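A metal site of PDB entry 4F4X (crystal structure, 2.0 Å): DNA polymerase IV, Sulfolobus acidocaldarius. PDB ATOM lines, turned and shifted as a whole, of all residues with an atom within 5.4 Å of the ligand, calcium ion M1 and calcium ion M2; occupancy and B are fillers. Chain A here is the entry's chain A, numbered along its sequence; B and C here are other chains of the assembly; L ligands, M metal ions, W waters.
OG1 of Thr 45 is in hydrogen-bond range of O9 of the ligand (2.5 Å). N of Tyr 10 is in hydrogen-bond range of O11 of the ligand (2.8 Å). An oxygen (O11) of the ligand lies within salt-bridge range of the side-chain amino group of Lys 160 (3.5 Å). OH of Tyr 48 is in hydrogen-bond range of O11 of the ligand. N of Phe 12 lies within hydrogen-bond range of O3 of the ligand (3.4 Å). The backbone NH of Phe 11 sits close to an oxygen (O8) of the ligand, 3.1 Å away. The guanidinium group of Arg 51 is in salt-bridge range of an oxygen (O12) of the ligand, 3.0 Å away. O6 of DG 5 of chain C is in hydrogen-bond range of a nitrogen (N3) of the ligand, 2.8 Å away.
The backbone carbonyl oxygen of Val 43 sits at hydrogen-bond distance from the backbone NH of Gly 58, 2.8 Å away. The backbone NH (N) of Asp 105 lies close to the side-chain hydroxyl (OG) of Ser 103, 3.1 Å away. The guanidinium group (NH2) of Arg 51 sits at hydrogen-bond distance from the side-chain hydroxyl (OG1) of Thr 45 (3.2 Å). The side-chain amino group (NZ) of Lys 160 lies within salt-bridge range of the side-chain carboxylate (OD2) of Asp 9 (3.2 Å). O2 of DC 6 of chain C lies close to N2 of DG 13 of chain B (2.6 Å). OE2 of Glu 106 is in salt-bridge range of NZ of Lys 153 (2.8 Å). O of Ala 46 is in hydrogen-bond range of NE of Arg 51 (2.8 Å). N of Glu 106 is in hydrogen-bond range of OG of Ser 103, at 3.4 Å.
N1 of the ligand lies close to O of Ala 44 (3.5 Å). Residues that only touch the ligand: Asp 9, Ala 57, Gly 58 and DG 13 of chain B. Hydrophobic or aromatic side chains that line the ligand: Phe 11, Phe 12, Ala 44, Tyr 48 and Ala 57. Within 4 Å of the ligand: Asp 7, Phe 8, Asp 9, Tyr 10, Phe 11, Phe 12, Ala 44, Thr 45, Tyr 48, Arg 51, Ala 57, Gly 58, Asp 105, Lys 160, DG 13 of chain B, DC 14 of chain B and DG 5 of chain C. Along chain A the residues within 4 Å of the ligand span positions 7 to 160. The nearest printed residue that does not touch the ligand is Val 43 (4.7 Å).
Residues that only touch calcium ion M1: Lys 160. The nearest printed residue that does not touch calcium ion M1 is Tyr 10 (4.6 Å).
The nearest printed residue that does not touch calcium ion M2 is Lys 153 (4.8 Å).
Calcium ion M1 is bound by the backbone carbonyl oxygen (O) of Phe 8, the side-chain carboxylate (OD2) of Asp 7, an oxygen (O8) of the ligand, an oxygen (O13) of the ligand, an oxygen (O6) of the ligand, the side-chain carboxylate (OD2) of Asp 105 and the side-chain carboxylate (OD1) of Asp 105.
Calcium ion M2 is bound by water W2 (2.3 Å), OP1 of DC 14 of chain B (2.5 Å), OE1 of Glu 106 (2.6 Å), O6 of the ligand (2.7 Å), OD1 of Asp 105 (2.7 Å) and OD1 of Asp 7 (2.8 Å). Calcium ion M2 has six donor atoms within binding distance.
Water W4 bridges a nitrogen (N3) of the ligand (2.9 Å) and the backbone carbonyl oxygen of Ala 57 (3.5 Å). Water W5 bridges O1 of the ligand (2.9 Å) and N2 of DG 13 of chain B (3.4 Å). Water W3 lies within hydrogen-bond range of the side-chain hydroxyl of Thr 45 (2.7 Å), an oxygen (O9) of the ligand (3.0 Å) and the backbone carbonyl oxygen of Ala 44 (3.5 Å).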
ATOM      1  N   ASP A   7      -9.139 -16.977  16.237  1.00  0.00           N
ATOM      2  CA  ASP A   7      -9.732 -17.321  14.958  1.00  0.00           C
ATOM      3  C   ASP A   7      -9.621 -16.085  14.039  1.00  0.00           C
ATOM      4  O   ASP A   7     -10.112 -15.019  14.394  1.00  0.00           O
ATOM      5  CB  ASP A   7     -11.173 -17.749  15.271  1.00  0.00           C
ATOM      6  CG  ASP A   7     -11.948 -18.161  14.076  1.00  0.00           C
ATOM      7  OD1 ASP A   7     -12.636 -19.192  14.125  1.00  0.00           O
ATOM      8  OD2 ASP A   7     -11.950 -17.411  13.115  1.00  0.00           O
ATOM      9  N   PHE A   8      -8.951 -16.206  12.887  1.00  0.00           N
ATOM     10  CA  PHE A   8      -8.615 -15.034  12.071  1.00  0.00           C
ATOM     11  C   PHE A   8      -9.826 -14.515  11.322  1.00  0.00           C
ATOM     12  O   PHE A   8     -10.502 -15.295  10.716  1.00  0.00           O
ATOM     13  CB  PHE A   8      -7.541 -15.358  11.029  1.00  0.00           C
ATOM     14  CG  PHE A   8      -6.312 -16.016  11.600  1.00  0.00           C
ATOM     15  CD1 PHE A   8      -5.513 -16.800  10.788  1.00  0.00           C
ATOM     16  CD2 PHE A   8      -5.942 -15.823  12.922  1.00  0.00           C
ATOM     17  CE1 PHE A   8      -4.359 -17.377  11.279  1.00  0.00           C
ATOM     18  CE2 PHE A   8      -4.789 -16.439  13.438  1.00  0.00           C
ATOM     19  CZ  PHE A   8      -4.005 -17.210  12.607  1.00  0.00           C
ATOM     20  N   ASP A   9     -10.102 -13.215  11.306  1.00  0.00           N
ATOM     21  CA  ASP A   9     -11.334 -12.764  10.612  1.00  0.00           C
ATOM     22  C   ASP A   9     -11.259 -12.885   9.087  1.00  0.00           C
ATOM     23  O   ASP A   9     -10.244 -12.540   8.482  1.00  0.00           O
ATOM     24  CB  ASP A   9     -11.679 -11.313  10.988  1.00  0.00           C
ATOM     25  CG  ASP A   9     -11.872 -11.120  12.483  1.00  0.00           C
ATOM     26  OD1 ASP A   9     -11.643  -9.993  12.956  1.00  0.00           O
ATOM     27  OD2 ASP A   9     -12.248 -12.082  13.195  1.00  0.00           O
ATOM     28  N   TYR A  10     -12.350 -13.356   8.481  1.00  0.00           N
ATOM     29  CA  TYR A  10     -12.480 -13.512   7.007  1.00  0.00           C
ATOM     30  C   TYR A  10     -11.136 -13.787   6.300  1.00  0.00           C
ATOM     31  O   TYR A  10     -10.766 -13.124   5.346  1.00  0.00           O
ATOM     32  CB  TYR A  10     -13.271 -12.327   6.363  1.00  0.00           C
ATOM     33  CG  TYR A  10     -12.645 -10.937   6.488  1.00  0.00           C
ATOM     34  CD1 TYR A  10     -12.065 -10.313   5.388  1.00  0.00           C
ATOM     35  CD2 TYR A  10     -12.663 -10.248   7.695  1.00  0.00           C
ATOM     36  CE1 TYR A  10     -11.494  -9.017   5.476  1.00  0.00           C
ATOM     37  CE2 TYR A  10     -12.090  -8.963   7.805  1.00  0.00           C
ATOM     38  CZ  TYR A  10     -11.509  -8.363   6.688  1.00  0.00           C
ATOM     39  OH  TYR A  10     -10.956  -7.107   6.784  1.00  0.00           O
ATOM     40  N   PHE A  11     -10.444 -14.820   6.797  1.00  0.00           N
ATOM     41  CA  PHE A  11      -8.999 -14.963   6.606  1.00  0.00           C
ATOM     42  C   PHE A  11      -8.469 -14.723   5.192  1.00  0.00           C
ATOM     43  O   PHE A  11      -7.692 -13.800   4.978  1.00  0.00           O
ATOM     44  CB  PHE A  11      -8.489 -16.306   7.161  1.00  0.00           C
ATOM     45  CG  PHE A  11      -6.971 -16.417   7.209  1.00  0.00           C
ATOM     46  CD1 PHE A  11      -6.211 -15.354   7.666  1.00  0.00           C
ATOM     47  CD2 PHE A  11      -6.325 -17.577   6.819  1.00  0.00           C
ATOM     48  CE1 PHE A  11      -4.812 -15.417   7.708  1.00  0.00           C
ATOM     49  CE2 PHE A  11      -4.936 -17.662   6.856  1.00  0.00           C
ATOM     50  CZ  PHE A  11      -4.178 -16.588   7.291  1.00  0.00           C
ATOM     51  N   PHE A  12      -8.871 -15.553   4.225  1.00  0.00           N
ATOM     52  CA  PHE A  12      -8.264 -15.444   2.898  1.00  0.00           C
ATOM     53  C   PHE A  12      -8.494 -14.057   2.296  1.00  0.00           C
ATOM     54  O   PHE A  12      -7.578 -13.471   1.696  1.00  0.00           O
ATOM     55  CB  PHE A  12      -8.737 -16.548   1.933  1.00  0.00           C
ATOM     56  CG  PHE A  12      -8.330 -17.961   2.352  1.00  0.00           C
ATOM     57  CD1 PHE A  12      -7.594 -18.193   3.505  1.00  0.00           C
ATOM     58  CD2 PHE A  12      -8.686 -19.061   1.570  1.00  0.00           C
ATOM     59  CE1 PHE A  12      -7.229 -19.498   3.895  1.00  0.00           C
ATOM     60  CE2 PHE A  12      -8.315 -20.362   1.949  1.00  0.00           C
ATOM     61  CZ  PHE A  12      -7.581 -20.557   3.107  1.00  0.00           C
ATOM     62  N   ALA A  13      -9.707 -13.513   2.448  1.00  0.00           N
ATOM     63  CA  ALA A  13     -10.010 -12.184   1.930  1.00  0.00           C
ATOM     64  C   ALA A  13      -9.225 -11.113   2.668  1.00  0.00           C
ATOM     65  O   ALA A  13      -8.794 -10.134   2.057  1.00  0.00           O
ATOM     66  CB  ALA A  13     -11.584 -11.876   1.996  1.00  0.00           C
ATOM     67  N   VAL A  43     -16.704 -20.056  -4.210  1.00  0.00           N
ATOM     68  CA  VAL A  43     -16.228 -19.013  -3.309  1.00  0.00           C
ATOM     69  C   VAL A  43     -15.535 -19.636  -2.112  1.00  0.00           C
ATOM     70  O   VAL A  43     -16.125 -20.487  -1.429  1.00  0.00           O
ATOM     71  CB  VAL A  43     -17.398 -18.116  -2.826  1.00  0.00           C
ATOM     72  CG1 VAL A  43     -16.937 -17.149  -1.736  1.00  0.00           C
ATOM     73  CG2 VAL A  43     -18.030 -17.367  -4.011  1.00  0.00           C
ATOM     74  N   ALA A  44     -14.278 -19.252  -1.883  1.00  0.00           N
ATOM     75  CA  ALA A  44     -13.525 -19.751  -0.725  1.00  0.00           C
ATOM     76  C   ALA A  44     -13.906 -18.941   0.510  1.00  0.00           C
ATOM     77  O   ALA A  44     -14.090 -19.494   1.589  1.00  0.00           O
ATOM     78  CB  ALA A  44     -11.994 -19.672  -0.963  1.00  0.00           C
ATOM     79  N   THR A  45     -14.000 -17.624   0.356  1.00  0.00           N
ATOM     80  CA  THR A  45     -14.474 -16.773   1.427  1.00  0.00           C
ATOM     81  C   THR A  45     -14.784 -15.373   0.900  1.00  0.00           C
ATOM     82  O   THR A  45     -14.396 -15.003  -0.200  1.00  0.00           O
ATOM     83  CB  THR A  45     -13.493 -16.682   2.591  1.00  0.00           C
ATOM     84  OG1 THR A  45     -14.171 -16.198   3.763  1.00  0.00           O
ATOM     85  CG2 THR A  45     -12.328 -15.784   2.248  1.00  0.00           C
ATOM     86  N   ALA A  46     -15.495 -14.583   1.674  1.00  0.00           N
ATOM     87  CA  ALA A  46     -15.820 -13.233   1.229  1.00  0.00           C
ATOM     88  C   ALA A  46     -15.635 -12.331   2.409  1.00  0.00           C
ATOM     89  O   ALA A  46     -15.910 -12.740   3.524  1.00  0.00           O
ATOM     90  CB  ALA A  46     -17.249 -13.180   0.752  1.00  0.00           C
ATOM     91  N   TYR A  48     -16.680  -9.175   4.891  1.00  0.00           N
ATOM     92  CA  TYR A  48     -17.993  -8.889   5.468  1.00  0.00           C
ATOM     93  C   TYR A  48     -18.863  -7.984   4.601  1.00  0.00           C
ATOM     94  O   TYR A  48     -20.073  -8.153   4.579  1.00  0.00           O
ATOM     95  CB  TYR A  48     -17.858  -8.358   6.896  1.00  0.00           C
ATOM     96  CG  TYR A  48     -17.616  -9.493   7.859  1.00  0.00           C
ATOM     97  CD1 TYR A  48     -18.655 -10.061   8.582  1.00  0.00           C
ATOM     98  CD2 TYR A  48     -16.343 -10.040   7.995  1.00  0.00           C
ATOM     99  CE1 TYR A  48     -18.432 -11.121   9.456  1.00  0.00           C
ATOM    100  CE2 TYR A  48     -16.110 -11.105   8.847  1.00  0.00           C
ATOM    101  CZ  TYR A  48     -17.146 -11.645   9.565  1.00  0.00           C
ATOM    102  OH  TYR A  48     -16.896 -12.696  10.422  1.00  0.00           O
ATOM    103  N   ARG A  51     -20.470 -10.283   2.230  1.00  0.00           N
ATOM    104  CA  ARG A  51     -21.417 -11.161   2.920  1.00  0.00           C
ATOM    105  C   ARG A  51     -22.734 -10.432   3.125  1.00  0.00           C
ATOM    106  O   ARG A  51     -23.805 -11.052   3.112  1.00  0.00           O
ATOM    107  CB  ARG A  51     -20.862 -11.638   4.264  1.00  0.00           C
ATOM    108  CG  ARG A  51     -19.672 -12.622   4.098  1.00  0.00           C
ATOM    109  CD  ARG A  51     -19.145 -13.083   5.435  1.00  0.00           C
ATOM    110  NE  ARG A  51     -17.825 -13.670   5.312  1.00  0.00           N
ATOM    111  CZ  ARG A  51     -17.184 -14.296   6.282  1.00  0.00           C
ATOM    112  NH1 ARG A  51     -17.749 -14.424   7.481  1.00  0.00           N
ATOM    113  NH2 ARG A  51     -15.972 -14.816   6.066  1.00  0.00           N
ATOM    114  N   ALA A  57     -19.369 -18.551   1.466  1.00  0.00           N
ATOM    115  CA  ALA A  57     -18.364 -19.592   1.189  1.00  0.00           C
ATOM    116  C   ALA A  57     -19.046 -20.874   0.719  1.00  0.00           C
ATOM    117  O   ALA A  57     -20.041 -21.305   1.291  1.00  0.00           O
ATOM    118  CB  ALA A  57     -17.564 -19.887   2.431  1.00  0.00           C
ATOM    119  N   GLY A  58     -18.510 -21.471  -0.349  1.00  0.00           N
ATOM    120  CA  GLY A  58     -19.050 -22.692  -0.926  1.00  0.00           C
ATOM    121  C   GLY A  58     -19.874 -22.416  -2.171  1.00  0.00           C
ATOM    122  O   GLY A  58     -20.037 -23.261  -3.035  1.00  0.00           O
ATOM    123  N   MET A  76      -7.918 -17.516  -5.529  1.00  0.00           N
ATOM    124  CA  MET A  76      -7.317 -17.982  -4.308  1.00  0.00           C
ATOM    125  C   MET A  76      -5.802 -18.172  -4.525  1.00  0.00           C
ATOM    126  O   MET A  76      -5.372 -18.688  -5.555  1.00  0.00           O
ATOM    127  CB  MET A  76      -7.969 -19.291  -3.865  1.00  0.00           C
ATOM    128  CG  MET A  76      -7.695 -19.633  -2.397  1.00  0.00           C
ATOM    129  SD  MET A  76      -8.306 -21.240  -1.909  1.00  0.00           S
ATOM    130  CE  MET A  76      -7.568 -22.265  -3.177  1.00  0.00           C
ATOM    131  N   SER A 103      -6.119 -25.461  12.579  1.00  0.00           N
ATOM    132  CA  SER A 103      -6.208 -25.329  11.129  1.00  0.00           C
ATOM    133  C   SER A 103      -5.399 -24.075  10.717  1.00  0.00           C
ATOM    134  O   SER A 103      -4.810 -23.415  11.551  1.00  0.00           O
ATOM    135  CB  SER A 103      -7.658 -25.153  10.689  1.00  0.00           C
ATOM    136  OG  SER A 103      -8.117 -23.832  10.950  1.00  0.00           O
ATOM    137  N   ILE A 104      -5.402 -23.760   9.430  1.00  0.00           N
ATOM    138  CA  ILE A 104      -4.671 -22.619   8.895  1.00  0.00           C
ATOM    139  C   ILE A 104      -5.205 -21.318   9.511  1.00  0.00           C
ATOM    140  O   ILE A 104      -4.551 -20.277   9.507  1.00  0.00           O
ATOM    141  CB  ILE A 104      -4.833 -22.597   7.350  1.00  0.00           C
ATOM    142  CG1 ILE A 104      -3.932 -21.588   6.680  1.00  0.00           C
ATOM    143  CG2 ILE A 104      -6.264 -22.316   6.943  1.00  0.00           C
ATOM    144  CD1 ILE A 104      -4.224 -21.529   5.195  1.00  0.00           C
ATOM    145  N   ASP A 105      -6.395 -21.406  10.079  1.00  0.00           N
ATOM    146  CA  ASP A 105      -7.167 -20.245  10.492  1.00  0.00           C
ATOM    147  C   ASP A 105      -7.316 -20.093  12.026  1.00  0.00           C
ATOM    148  O   ASP A 105      -7.685 -19.044  12.526  1.00  0.00           O
ATOM    149  CB  ASP A 105      -8.538 -20.389   9.858  1.00  0.00           C
ATOM    150  CG  ASP A 105      -9.433 -19.298  10.242  1.00  0.00           C
ATOM    151  OD1 ASP A 105      -9.982 -19.388  11.330  1.00  0.00           O
ATOM    152  OD2 ASP A 105      -9.544 -18.315   9.493  1.00  0.00           O
ATOM    153  N   GLU A 106      -7.024 -21.149  12.794  1.00  0.00           N
ATOM    154  CA  GLU A 106      -7.339 -21.078  14.217  1.00  0.00           C
ATOM    155  C   GLU A 106      -6.490 -21.961  15.115  1.00  0.00           C
ATOM    156  O   GLU A 106      -5.953 -22.978  14.693  1.00  0.00           O
ATOM    157  CB  GLU A 106      -8.838 -21.387  14.432  1.00  0.00           C
ATOM    158  CG  GLU A 106      -9.202 -22.875  14.396  1.00  0.00           C
ATOM    159  CD  GLU A 106     -10.710 -23.089  14.393  1.00  0.00           C
ATOM    160  OE1 GLU A 106     -11.392 -22.367  13.673  1.00  0.00           O
ATOM    161  OE2 GLU A 106     -11.259 -23.958  15.123  1.00  0.00           O
ATOM    162  N   LYS A 153     -14.238 -21.513  21.900  1.00  0.00           N
ATOM    163  CA  LYS A 153     -14.625 -21.387  20.494  1.00  0.00           C
ATOM    164  C   LYS A 153     -16.024 -20.801  20.304  1.00  0.00           C
ATOM    165  O   LYS A 153     -16.230 -19.956  19.438  1.00  0.00           O
ATOM    166  CB  LYS A 153     -14.509 -22.739  19.787  1.00  0.00           C
ATOM    167  CG  LYS A 153     -14.887 -22.697  18.319  1.00  0.00           C
ATOM    168  CD  LYS A 153     -14.750 -24.095  17.697  1.00  0.00           C
ATOM    169  CE  LYS A 153     -15.007 -24.083  16.202  1.00  0.00           C
ATOM    170  NZ  LYS A 153     -13.990 -23.277  15.468  1.00  0.00           N
ATOM    171  N   LYS A 160     -17.711 -12.403  16.709  1.00  0.00           N
ATOM    172  CA  LYS A 160     -17.173 -11.978  15.420  1.00  0.00           C
ATOM    173  C   LYS A 160     -17.878 -10.751  14.825  1.00  0.00           C
ATOM    174  O   LYS A 160     -19.088 -10.588  14.980  1.00  0.00           O
ATOM    175  CB  LYS A 160     -17.211 -13.133  14.414  1.00  0.00           C
ATOM    176  CG  LYS A 160     -16.390 -14.332  14.860  1.00  0.00           C
ATOM    177  CD  LYS A 160     -15.960 -15.167  13.682  1.00  0.00           C
ATOM    178  CE  LYS A 160     -14.836 -14.493  12.958  1.00  0.00           C
ATOM    179  NZ  LYS A 160     -13.478 -15.087  13.208  1.00  0.00           N
ATOM    180  P    DG B  13     -18.025 -25.466   8.922  1.00  0.00           P
ATOM    181  OP1  DG B  13     -18.374 -25.882  10.299  1.00  0.00           O
ATOM    182  OP2  DG B  13     -18.770 -24.437   8.189  1.00  0.00           O
ATOM    183  O5'  DG B  13     -16.491 -24.977   8.952  1.00  0.00           O
ATOM    184  C5'  DG B  13     -15.489 -25.866   9.464  1.00  0.00           C
ATOM    185  C4'  DG B  13     -14.130 -25.682   8.800  1.00  0.00           C
ATOM    186  O4'  DG B  13     -14.051 -26.272   7.486  1.00  0.00           O
ATOM    187  C3'  DG B  13     -13.639 -24.271   8.526  1.00  0.00           C
ATOM    188  O3'  DG B  13     -12.256 -24.438   8.546  1.00  0.00           O
ATOM    189  C2'  DG B  13     -14.140 -23.969   7.116  1.00  0.00           C
ATOM    190  C1'  DG B  13     -13.755 -25.298   6.500  1.00  0.00           C
ATOM    191  N9   DG B  13     -14.545 -25.747   5.374  1.00  0.00           N
ATOM    192  C8   DG B  13     -15.904 -25.970   5.366  1.00  0.00           C
ATOM    193  N7   DG B  13     -16.343 -26.410   4.216  1.00  0.00           N
ATOM    194  C5   DG B  13     -15.182 -26.498   3.432  1.00  0.00           C
ATOM    195  C6   DG B  13     -15.014 -26.928   2.099  1.00  0.00           C
ATOM    196  O6   DG B  13     -15.900 -27.325   1.322  1.00  0.00           O
ATOM    197  N1   DG B  13     -13.672 -26.860   1.681  1.00  0.00           N
ATOM    198  C2   DG B  13     -12.612 -26.464   2.468  1.00  0.00           C
ATOM    199  N2   DG B  13     -11.391 -26.466   1.897  1.00  0.00           N
ATOM    200  N3   DG B  13     -12.768 -26.063   3.721  1.00  0.00           N
ATOM    201  C4   DG B  13     -14.063 -26.107   4.137  1.00  0.00           C
ATOM    202  P    DC B  14     -11.421 -23.749   9.711  1.00  0.00           P
ATOM    203  OP1  DC B  14     -12.101 -22.526  10.026  1.00  0.00           O
ATOM    204  OP2  DC B  14     -10.005 -23.609   9.248  1.00  0.00           O
ATOM    205  O5'  DC B  14     -11.458 -24.823  10.911  1.00  0.00           O
ATOM    206  C5'  DC B  14     -12.455 -24.924  11.959  1.00  0.00           C
ATOM    207  C4'  DC B  14     -12.384 -26.296  12.638  1.00  0.00           C
ATOM    208  O4'  DC B  14     -12.761 -27.286  11.639  1.00  0.00           O
ATOM    209  C3'  DC B  14     -11.033 -26.781  13.202  1.00  0.00           C
ATOM    210  O3'  DC B  14     -11.160 -27.492  14.448  1.00  0.00           O
ATOM    211  C2'  DC B  14     -10.516 -27.763  12.143  1.00  0.00           C
ATOM    212  C1'  DC B  14     -11.829 -28.371  11.658  1.00  0.00           C
ATOM    213  N1   DC B  14     -11.716 -28.973  10.298  1.00  0.00           N
ATOM    214  C2   DC B  14     -12.159 -30.282  10.076  1.00  0.00           C
ATOM    215  O2   DC B  14     -12.647 -30.910  11.037  1.00  0.00           O
ATOM    216  N3   DC B  14     -12.034 -30.810   8.826  1.00  0.00           N
ATOM    217  C4   DC B  14     -11.507 -30.074   7.843  1.00  0.00           C
ATOM    218  N4   DC B  14     -11.422 -30.621   6.624  1.00  0.00           N
ATOM    219  C5   DC B  14     -11.071 -28.732   8.041  1.00  0.00           C
ATOM    220  C6   DC B  14     -11.181 -28.231   9.272  1.00  0.00           C
ATOM    221  P    DG C   5     -16.542 -26.306 -10.425  1.00  0.00           P
ATOM    222  OP1  DG C   5     -16.233 -25.948 -11.827  1.00  0.00           O
ATOM    223  OP2  DG C   5     -16.839 -27.690 -10.047  1.00  0.00           O
ATOM    224  O5'  DG C   5     -15.318 -25.729  -9.571  1.00  0.00           O
ATOM    225  C5'  DG C   5     -15.413 -25.611  -8.165  1.00  0.00           C
ATOM    226  C4'  DG C   5     -14.003 -25.347  -7.699  1.00  0.00           C
ATOM    227  O4'  DG C   5     -13.970 -24.936  -6.317  1.00  0.00           O
ATOM    228  C3'  DG C   5     -13.198 -26.649  -7.759  1.00  0.00           C
ATOM    229  O3'  DG C   5     -11.875 -26.276  -8.002  1.00  0.00           O
ATOM    230  C2'  DG C   5     -13.464 -27.254  -6.390  1.00  0.00           C
ATOM    231  C1'  DG C   5     -13.464 -26.001  -5.515  1.00  0.00           C
ATOM    232  N9   DG C   5     -14.373 -25.904  -4.389  1.00  0.00           N
ATOM    233  C8   DG C   5     -15.688 -26.296  -4.349  1.00  0.00           C
ATOM    234  N7   DG C   5     -16.246 -26.036  -3.197  1.00  0.00           N
ATOM    235  C5   DG C   5     -15.262 -25.408  -2.441  1.00  0.00           C
ATOM    236  C6   DG C   5     -15.289 -24.866  -1.129  1.00  0.00           C
ATOM    237  O6   DG C   5     -16.232 -24.846  -0.324  1.00  0.00           O
ATOM    238  N1   DG C   5     -14.072 -24.295  -0.755  1.00  0.00           N
ATOM    239  C2   DG C   5     -12.947 -24.271  -1.538  1.00  0.00           C
ATOM    240  N2   DG C   5     -11.853 -23.697  -0.999  1.00  0.00           N
ATOM    241  N3   DG C   5     -12.917 -24.760  -2.787  1.00  0.00           N
ATOM    242  C4   DG C   5     -14.104 -25.307  -3.169  1.00  0.00           C
ATOM    243  P    DC C   6     -10.749 -27.400  -8.228  1.00  0.00           P
ATOM    244  OP1  DC C   6      -9.680 -26.795  -9.013  1.00  0.00           O
ATOM    245  OP2  DC C   6     -11.431 -28.656  -8.671  1.00  0.00           O
ATOM    246  O5'  DC C   6     -10.217 -27.691  -6.773  1.00  0.00           O
ATOM    247  C5'  DC C   6      -9.180 -26.841  -6.305  1.00  0.00           C
ATOM    248  C4'  DC C   6      -8.961 -27.291  -4.873  1.00  0.00           C
ATOM    249  O4'  DC C   6     -10.220 -27.179  -4.178  1.00  0.00           O
ATOM    250  C3'  DC C   6      -8.497 -28.736  -4.654  1.00  0.00           C
ATOM    251  O3'  DC C   6      -7.290 -28.594  -3.960  1.00  0.00           O
ATOM    252  C2'  DC C   6      -9.529 -29.311  -3.706  1.00  0.00           C
ATOM    253  C1'  DC C   6     -10.143 -28.061  -3.098  1.00  0.00           C
ATOM    254  N1   DC C   6     -11.517 -28.231  -2.577  1.00  0.00           N
ATOM    255  C2   DC C   6     -11.838 -27.744  -1.296  1.00  0.00           C
ATOM    256  O2   DC C   6     -10.972 -27.159  -0.615  1.00  0.00           O
ATOM    257  N3   DC C   6     -13.113 -27.900  -0.847  1.00  0.00           N
ATOM    258  C4   DC C   6     -14.017 -28.516  -1.609  1.00  0.00           C
ATOM    259  N4   DC C   6     -15.249 -28.663  -1.118  1.00  0.00           N
ATOM    260  C5   DC C   6     -13.703 -29.035  -2.905  1.00  0.00           C
ATOM    261  C6   DC C   6     -12.452 -28.859  -3.343  1.00  0.00           C
HETATM  262  N1  LIG L   1     -12.610 -21.930   3.553  1.00  0.00           N
HETATM  263  C1  LIG L   1     -12.715 -22.499   2.341  1.00  0.00           C
HETATM  264  N2  LIG L   1     -13.867 -23.018   1.886  1.00  0.00           N
HETATM  265  C2  LIG L   1     -14.977 -22.966   2.655  1.00  0.00           C
HETATM  266  C3  LIG L   1     -14.927 -22.363   3.904  1.00  0.00           C
HETATM  267  C4  LIG L   1     -13.703 -21.826   4.342  1.00  0.00           C
HETATM  268  O1  LIG L   1     -11.614 -22.571   1.576  1.00  0.00           O
HETATM  269  N3  LIG L   1     -16.213 -23.488   2.176  1.00  0.00           N
HETATM  270  C5  LIG L   1     -11.329 -21.347   3.995  1.00  0.00           C
HETATM  271  C6  LIG L   1     -11.324 -19.901   3.681  1.00  0.00           C
HETATM  272  C7  LIG L   1     -11.640 -19.244   4.988  1.00  0.00           C
HETATM  273  C8  LIG L   1     -10.903 -20.087   5.880  1.00  0.00           C
HETATM  274  O2  LIG L   1     -11.200 -21.421   5.379  1.00  0.00           O
HETATM  275  O3  LIG L   1     -11.238 -17.891   5.057  1.00  0.00           O
HETATM  276  C9  LIG L   1     -11.383 -19.955   7.263  1.00  0.00           C
HETATM  277  O4  LIG L   1     -12.680 -20.423   7.515  1.00  0.00           O
HETATM  278  P1  LIG L   1     -13.751 -19.689   8.383  1.00  0.00           P
HETATM  279  O5  LIG L   1     -14.859 -20.605   8.780  1.00  0.00           O
HETATM  280  O6  LIG L   1     -13.212 -19.463   9.700  1.00  0.00           O
HETATM  281  O7  LIG L   1     -14.365 -18.402   7.722  1.00  0.00           O
HETATM  282  P2  LIG L   1     -13.636 -17.033   7.524  1.00  0.00           P
HETATM  283  O8  LIG L   1     -12.274 -16.972   8.038  1.00  0.00           O
HETATM  284  O9  LIG L   1     -13.398 -16.769   6.077  1.00  0.00           O
HETATM  285  O10 LIG L   1     -14.558 -15.887   8.100  1.00  0.00           O
HETATM  286  P3  LIG L   1     -14.946 -15.644   9.603  1.00  0.00           P
HETATM  287  O11 LIG L   1     -14.578 -14.228   9.988  1.00  0.00           O
HETATM  288  O12 LIG L   1     -16.412 -15.798   9.769  1.00  0.00           O
HETATM  289  O13 LIG L   1     -14.307 -16.527  10.673  1.00  0.00           O
HETATM  290 CA    CA M   1     -11.851 -17.399  10.570  1.00  0.00          CA
HETATM  291 CA    CA M   2     -12.269 -20.730  11.828  1.00  0.00          CA
HETATM  292  O   HOH W   1     -16.477 -20.398   6.446  1.00  0.00           O
HETATM  293  O   HOH W   2     -14.537 -21.162  11.995  1.00  0.00           O
HETATM  294  O   HOH W   3     -15.423 -18.403   4.599  1.00  0.00           O
HETATM  295  O   HOH W   4     -18.649 -23.338   3.726  1.00  0.00           O
HETATM  296  O   HOH W   5      -9.052 -23.986   1.614  1.00  0.00           O
